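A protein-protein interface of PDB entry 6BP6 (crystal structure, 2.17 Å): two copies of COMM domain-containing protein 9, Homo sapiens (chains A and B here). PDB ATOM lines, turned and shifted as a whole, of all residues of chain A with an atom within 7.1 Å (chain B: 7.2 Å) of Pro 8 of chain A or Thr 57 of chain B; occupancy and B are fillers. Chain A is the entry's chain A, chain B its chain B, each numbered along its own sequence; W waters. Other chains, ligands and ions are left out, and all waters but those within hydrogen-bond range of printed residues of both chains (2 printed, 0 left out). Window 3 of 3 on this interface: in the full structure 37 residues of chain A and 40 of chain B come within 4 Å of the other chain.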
ATOM      1  N   SER A   6      26.092  -7.938  -4.421  1.00  0.00           N
ATOM      2  CA  SER A   6      25.547  -6.773  -3.725  1.00  0.00           C
ATOM      3  C   SER A   6      26.644  -5.731  -3.506  1.00  0.00           C
ATOM      4  O   SER A   6      27.312  -5.717  -2.471  1.00  0.00           O
ATOM      5  CB  SER A   6      24.913  -7.195  -2.397  1.00  0.00           C
ATOM      6  OG  SER A   6      24.363  -6.078  -1.715  1.00  0.00           O
ATOM      7  N   LEU A   7      26.815  -4.846  -4.489  1.00  0.00           N
ATOM      8  CA  LEU A   7      27.647  -3.667  -4.309  1.00  0.00           C
ATOM      9  C   LEU A   7      26.936  -2.647  -3.417  1.00  0.00           C
ATOM     10  O   LEU A   7      25.710  -2.678  -3.278  1.00  0.00           O
ATOM     11  CB  LEU A   7      27.980  -3.032  -5.658  1.00  0.00           C
ATOM     12  CG  LEU A   7      29.124  -3.641  -6.468  1.00  0.00           C
ATOM     13  CD1 LEU A   7      29.639  -2.636  -7.491  1.00  0.00           C
ATOM     14  CD2 LEU A   7      30.255  -4.116  -5.554  1.00  0.00           C
ATOM     15  N   PRO A   8      27.686  -1.740  -2.789  1.00  0.00           N
ATOM     16  CA  PRO A   8      27.051  -0.732  -1.930  1.00  0.00           C
ATOM     17  C   PRO A   8      26.098   0.153  -2.719  1.00  0.00           C
ATOM     18  O   PRO A   8      26.418   0.636  -3.808  1.00  0.00           O
ATOM     19  CB  PRO A   8      28.242   0.064  -1.383  1.00  0.00           C
ATOM     20  CG  PRO A   8      29.369  -0.907  -1.416  1.00  0.00           C
ATOM     21  CD  PRO A   8      29.153  -1.724  -2.656  1.00  0.00           C
ATOM     22  N   ARG A   9      24.912   0.368  -2.157  1.00  0.00           N
ATOM     23  CA  ARG A   9      23.881   1.144  -2.830  1.00  0.00           C
ATOM     24  C   ARG A   9      23.447   2.310  -1.954  1.00  0.00           C
ATOM     25  O   ARG A   9      23.268   2.160  -0.740  1.00  0.00           O
ATOM     26  CB  ARG A   9      22.682   0.259  -3.203  1.00  0.00           C
ATOM     27  CG  ARG A   9      23.078  -0.953  -4.062  1.00  0.00           C
ATOM     28  CD  ARG A   9      21.893  -1.561  -4.805  1.00  0.00           C
ATOM     29  NE  ARG A   9      21.638  -0.902  -6.084  1.00  0.00           N
ATOM     30  CZ  ARG A   9      21.964  -1.405  -7.274  1.00  0.00           C
ATOM     31  NH1 ARG A   9      22.558  -2.591  -7.366  1.00  0.00           N
ATOM     32  NH2 ARG A   9      21.689  -0.723  -8.379  1.00  0.00           N
ATOM     33  N   LEU A  10      23.302   3.474  -2.576  1.00  0.00           N
ATOM     34  CA  LEU A  10      22.757   4.637  -1.895  1.00  0.00           C
ATOM     35  C   LEU A  10      21.264   4.448  -1.691  1.00  0.00           C
ATOM     36  O   LEU A  10      20.502   4.365  -2.658  1.00  0.00           O
ATOM     37  CB  LEU A  10      23.039   5.891  -2.717  1.00  0.00           C
ATOM     38  CG  LEU A  10      22.771   7.278  -2.128  1.00  0.00           C
ATOM     39  CD1 LEU A  10      22.921   7.287  -0.629  1.00  0.00           C
ATOM     40  CD2 LEU A  10      23.744   8.265  -2.748  1.00  0.00           C
ATOM     41  N   VAL A  11      20.844   4.360  -0.430  1.00  0.00           N
ATOM     42  CA  VAL A  11      19.455   4.079  -0.115  1.00  0.00           C
ATOM     43  C   VAL A  11      18.747   5.232   0.578  1.00  0.00           C
ATOM     44  O   VAL A  11      17.508   5.217   0.654  1.00  0.00           O
ATOM     45  CB  VAL A  11      19.315   2.795   0.728  1.00  0.00           C
ATOM     46  CG1 VAL A  11      19.930   1.619  -0.011  1.00  0.00           C
ATOM     47  CG2 VAL A  11      19.948   2.980   2.104  1.00  0.00           C
ATOM     48  N   ILE A  40      24.151   4.639   2.844  1.00  0.00           N
ATOM     49  CA  ILE A  40      24.602   3.596   1.928  1.00  0.00           C
ATOM     50  C   ILE A  40      24.331   2.240   2.566  1.00  0.00           C
ATOM     51  O   ILE A  40      24.759   1.987   3.699  1.00  0.00           O
ATOM     52  CB  ILE A  40      26.105   3.734   1.626  1.00  0.00           C
ATOM     53  CG1 ILE A  40      26.495   5.192   1.369  1.00  0.00           C
ATOM     54  CG2 ILE A  40      26.509   2.835   0.466  1.00  0.00           C
ATOM     55  CD1 ILE A  40      26.075   5.715   0.028  1.00  0.00           C
ATOM     56  N   GLN A  41      23.656   1.359   1.834  1.00  0.00           N
ATOM     57  CA  GLN A  41      23.387  -0.001   2.283  1.00  0.00           C
ATOM     58  C   GLN A  41      24.235  -0.982   1.485  1.00  0.00           C
ATOM     59  O   GLN A  41      24.402  -0.825   0.271  1.00  0.00           O
ATOM     60  CB  GLN A  41      21.902  -0.347   2.136  1.00  0.00           C
ATOM     61  CG  GLN A  41      21.534  -1.776   2.492  1.00  0.00           C
ATOM     62  CD  GLN A  41      20.053  -2.055   2.301  1.00  0.00           C
ATOM     63  OE1 GLN A  41      19.202  -1.308   2.784  1.00  0.00           O
ATOM     64  NE2 GLN A  41      19.739  -3.132   1.587  1.00  0.00           N
ATOM     65  N   GLU A  42      24.766  -1.994   2.164  1.00  0.00           N
ATOM     66  CA  GLU A  42      25.606  -2.994   1.513  1.00  0.00           C
ATOM     67  C   GLU A  42      25.026  -4.399   1.558  1.00  0.00           C
ATOM     68  O   GLU A  42      25.137  -5.129   0.571  1.00  0.00           O
ATOM     69  CB  GLU A  42      27.003  -3.003   2.147  1.00  0.00           C
ATOM     70  CG  GLU A  42      28.034  -3.776   1.346  1.00  0.00           C
ATOM     71  CD  GLU A  42      29.223  -4.199   2.184  1.00  0.00           C
ATOM     72  OE1 GLU A  42      29.023  -4.517   3.375  1.00  0.00           O
ATOM     73  OE2 GLU A  42      30.355  -4.210   1.656  1.00  0.00           O
ATOM     74  N   ASP A  43      24.408  -4.786   2.675  1.00  0.00           N
ATOM     75  CA  ASP A  43      23.878  -6.139   2.921  1.00  0.00           C
ATOM     76  C   ASP A  43      24.736  -7.261   2.337  1.00  0.00           C
ATOM     77  O   ASP A  43      24.309  -8.415   2.285  1.00  0.00           O
ATOM     78  CB  ASP A  43      22.444  -6.270   2.385  1.00  0.00           C
ATOM     79  CG  ASP A  43      22.385  -6.399   0.874  1.00  0.00           C
ATOM     80  OD1 ASP A  43      22.469  -5.365   0.178  1.00  0.00           O
ATOM     81  OD2 ASP A  43      22.256  -7.540   0.381  1.00  0.00           O
ATOM     82  N   SER A  54      25.550   2.411   6.451  1.00  0.00           N
ATOM     83  CA  SER A  54      26.513   3.424   6.851  1.00  0.00           C
ATOM     84  C   SER A  54      26.050   4.797   6.376  1.00  0.00           C
ATOM     85  O   SER A  54      25.171   4.919   5.521  1.00  0.00           O
ATOM     86  CB  SER A  54      27.902   3.104   6.296  1.00  0.00           C
ATOM     87  OG  SER A  54      27.822   2.686   4.948  1.00  0.00           O
ATOM     88  N   CYS B  34      25.402   2.248 -13.180  1.00  0.00           N
ATOM     89  CA  CYS B  34      26.442   3.229 -12.924  1.00  0.00           C
ATOM     90  C   CYS B  34      27.262   2.792 -11.718  1.00  0.00           C
ATOM     91  O   CYS B  34      26.711   2.332 -10.717  1.00  0.00           O
ATOM     92  CB  CYS B  34      25.821   4.608 -12.685  1.00  0.00           C
ATOM     93  SG  CYS B  34      26.978   5.886 -12.172  1.00  0.00           S
ATOM     94  N   LEU B  35      28.581   2.899 -11.829  1.00  0.00           N
ATOM     95  CA  LEU B  35      29.471   2.846 -10.678  1.00  0.00           C
ATOM     96  C   LEU B  35      29.928   4.272 -10.395  1.00  0.00           C
ATOM     97  O   LEU B  35      30.564   4.899 -11.247  1.00  0.00           O
ATOM     98  CB  LEU B  35      30.665   1.923 -10.935  1.00  0.00           C
ATOM     99  CG  LEU B  35      30.346   0.457 -11.237  1.00  0.00           C
ATOM    100  CD1 LEU B  35      31.618  -0.373 -11.411  1.00  0.00           C
ATOM    101  CD2 LEU B  35      29.474  -0.126 -10.140  1.00  0.00           C
ATOM    102  N   LEU B  36      29.570   4.795  -9.223  1.00  0.00           N
ATOM    103  CA  LEU B  36      29.859   6.169  -8.840  1.00  0.00           C
ATOM    104  C   LEU B  36      30.880   6.178  -7.712  1.00  0.00           C
ATOM    105  O   LEU B  36      30.711   5.487  -6.703  1.00  0.00           O
ATOM    106  CB  LEU B  36      28.587   6.892  -8.399  1.00  0.00           C
ATOM    107  CG  LEU B  36      28.742   8.341  -7.935  1.00  0.00           C
ATOM    108  CD1 LEU B  36      29.109   9.254  -9.100  1.00  0.00           C
ATOM    109  CD2 LEU B  36      27.474   8.823  -7.251  1.00  0.00           C
ATOM    110  N   GLN B  37      31.925   6.974  -7.874  1.00  0.00           N
ATOM    111  CA  GLN B  37      32.968   7.108  -6.872  1.00  0.00           C
ATOM    112  C   GLN B  37      33.062   8.562  -6.435  1.00  0.00           C
ATOM    113  O   GLN B  37      33.356   9.446  -7.245  1.00  0.00           O
ATOM    114  CB  GLN B  37      34.297   6.629  -7.433  1.00  0.00           C
ATOM    115  CG  GLN B  37      35.415   6.568  -6.438  1.00  0.00           C
ATOM    116  CD  GLN B  37      36.662   6.017  -7.075  1.00  0.00           C
ATOM    117  OE1 GLN B  37      37.593   6.761  -7.380  1.00  0.00           O
ATOM    118  NE2 GLN B  37      36.682   4.705  -7.302  1.00  0.00           N
ATOM    119  N   MET B  38      32.806   8.803  -5.159  1.00  0.00           N
ATOM    120  CA  MET B  38      32.968  10.114  -4.557  1.00  0.00           C
ATOM    121  C   MET B  38      34.199  10.121  -3.665  1.00  0.00           C
ATOM    122  O   MET B  38      34.399   9.217  -2.863  1.00  0.00           O
ATOM    123  CB  MET B  38      31.727  10.480  -3.755  1.00  0.00           C
ATOM    124  CG  MET B  38      30.488  10.634  -4.613  1.00  0.00           C
ATOM    125  SD  MET B  38      28.862  10.683  -3.544  1.00  0.00           S
ATOM    126  CE  MET B  38      28.894   8.853  -2.851  1.00  0.00           C
ATOM    127  N   ALA B  55      37.386   7.307  -0.215  1.00  0.00           N
ATOM    128  CA  ALA B  55      36.620   7.038  -1.426  1.00  0.00           C
ATOM    129  C   ALA B  55      35.386   6.219  -1.080  1.00  0.00           C
ATOM    130  O   ALA B  55      35.480   5.208  -0.378  1.00  0.00           O
ATOM    131  CB  ALA B  55      37.469   6.302  -2.468  1.00  0.00           C
ATOM    132  N   VAL B  56      34.237   6.666  -1.574  1.00  0.00           N
ATOM    133  CA  VAL B  56      32.956   6.004  -1.382  1.00  0.00           C
ATOM    134  C   VAL B  56      32.448   5.618  -2.763  1.00  0.00           C
ATOM    135  O   VAL B  56      32.148   6.490  -3.586  1.00  0.00           O
ATOM    136  CB  VAL B  56      31.950   6.912  -0.666  1.00  0.00           C
ATOM    137  CG1 VAL B  56      30.593   6.248  -0.601  1.00  0.00           C
ATOM    138  CG2 VAL B  56      32.456   7.269   0.725  1.00  0.00           C
ATOM    139  N   THR B  57      32.349   4.321  -3.024  1.00  0.00           N
ATOM    140  CA  THR B  57      31.891   3.813  -4.308  1.00  0.00           C
ATOM    141  C   THR B  57      30.545   3.123  -4.130  1.00  0.00           C
ATOM    142  O   THR B  57      30.398   2.255  -3.264  1.00  0.00           O
ATOM    143  CB  THR B  57      32.920   2.850  -4.906  1.00  0.00           C
ATOM    144  OG1 THR B  57      34.093   3.583  -5.278  1.00  0.00           O
ATOM    145  CG2 THR B  57      32.359   2.152  -6.129  1.00  0.00           C
ATOM    146  N   VAL B  58      29.565   3.520  -4.940  1.00  0.00           N
ATOM    147  CA  VAL B  58      28.223   2.957  -4.893  1.00  0.00           C
ATOM    148  C   VAL B  58      27.792   2.582  -6.305  1.00  0.00           C
ATOM    149  O   VAL B  58      28.308   3.097  -7.298  1.00  0.00           O
ATOM    150  CB  VAL B  58      27.194   3.924  -4.261  1.00  0.00           C
ATOM    151  CG1 VAL B  58      27.618   4.316  -2.860  1.00  0.00           C
ATOM    152  CG2 VAL B  58      27.001   5.159  -5.130  1.00  0.00           C
ATOM    153  N   GLU B  59      26.834   1.669  -6.387  1.00  0.00           N
ATOM    154  CA  GLU B  59      26.211   1.305  -7.651  1.00  0.00           C
ATOM    155  C   GLU B  59      24.846   1.969  -7.733  1.00  0.00           C
ATOM    156  O   GLU B  59      24.030   1.824  -6.818  1.00  0.00           O
ATOM    157  CB  GLU B  59      26.078  -0.213  -7.788  1.00  0.00           C
ATOM    158  CG  GLU B  59      25.422  -0.644  -9.087  1.00  0.00           C
ATOM    159  CD  GLU B  59      25.667  -2.107  -9.412  1.00  0.00           C
ATOM    160  OE1 GLU B  59      26.344  -2.792  -8.621  1.00  0.00           O
ATOM    161  OE2 GLU B  59      25.183  -2.576 -10.463  1.00  0.00           O
ATOM    162  N   LEU B  60      24.606   2.695  -8.828  1.00  0.00           N
ATOM    163  CA  LEU B  60      23.398   3.484  -9.035  1.00  0.00           C
ATOM    164  C   LEU B  60      22.599   2.955 -10.218  1.00  0.00           C
ATOM    165  O   LEU B  60      23.157   2.703 -11.295  1.00  0.00           O
ATOM    166  CB  LEU B  60      23.726   4.955  -9.300  1.00  0.00           C
ATOM    167  CG  LEU B  60      24.319   5.827  -8.204  1.00  0.00           C
ATOM    168  CD1 LEU B  60      24.431   7.255  -8.711  1.00  0.00           C
ATOM    169  CD2 LEU B  60      23.440   5.760  -6.979  1.00  0.00           C
HETATM  170  O   HOH W   1      22.345   3.219  -5.056  1.00  0.00           O
HETATM  171  O   HOH W   2      25.367  -4.989  -6.453  1.00  0.00           O
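The side-chain carboxylate (OE1) of Glu 59 of chain B is in salt-bridge range of the guanidinium group (NH1) of Arg 9 of chain A (3.99 Å). O of Pro 8 of chain A sits at hydrogen-bond distance from N of Glu 59 of chain B, 2.8 Å away.
The backbone NH of Leu 36 of chain B lies within hydrogen-bond range of the backbone carbonyl oxygen of Val 58 of chain B, at 2.9 Å. O of Arg 9 of chain A lies within hydrogen-bond range of N of Gln 41 of chain A (2.7 Å). The backbone NH (N) of Ile 40 of chain A lies within hydrogen-bond range of the backbone carbonyl oxygen (O) of Ser 54 of chain A (2.9 Å). The side-chain amide nitrogen (NE2) of Gln 37 of chain B lies close to the side-chain hydroxyl (OG1) of Thr 57 of chain B (3.5 Å).
Among the printed residues, pairs that only touch across the chains: Leu 7 of chain A with Leu 35 of chain B (3.7 Å), Leu 7 of chain A with Glu 59 of chain B (3.4 Å), Pro 8 of chain A with Thr 57 of chain B (3.6 Å), Pro 8 of chain A with Val 58 of chain B (3.1 Å) and Ile 40 of chain A with Val 58 of chain B (3.6 Å).
Pro 8 of chain A touches just these residues of chain B: Thr 57, Val 58 and Glu 59. Of chain A, only Pro 8 comes within 4 Å of Thr 57 of chain B. Of the printed residues of chain B, Arg 9 of chain A touches Glu 59. Of the printed residues of chain A, Val 58 of chain B touches Pro 8 and Ile 40. Of the printed residues of chain B, Ile 40 of chain A touches Val 58. Leu 10 of chain A touches none of the printed residues of chain B. Gln 41 of chain A touches none of the printed residues of chain B. The nearest residue of chain B that does not touch Pro 8 of chain A is Leu 60 of chain B (5.7 Å).
Of the 11 printed residues of chain B, 4 touch a printed residue of chain A. Printed residues of chain B that touch a printed residue of chain A: Leu 35, Thr 57, Val 58 and Glu 59. Hydrophobic or aromatic side chains of chain B that line the printed part of chain A: Leu 35 and Val 58. Along chain B the printed residues that touch a printed residue of chain A span positions 35 to 59. Among the printed residues, 7 pairs touch across the chains. Among the printed residues, Asp or Glu carboxylates within 4 Å of a Lys or Arg side-chain nitrogen of the other chain: Arg 9 of chain A with Glu 59 of chain B.
No position is printed for both chains. Of the 7 pairs that touch across the chains among the printed residues, none has its exchanged pair printed and touching as well.
Water W2 lies within hydrogen-bond range of the backbone NH of Leu 7 of chain A (2.4 Å) and the side-chain carboxylate of Glu 59 of chain B (3.2 Å). Water W1 bridges the backbone NH of Leu 10 of chain A (2.7 Å) and the backbone carbonyl oxygen of Glu 59 of chain B (2.8 Å).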
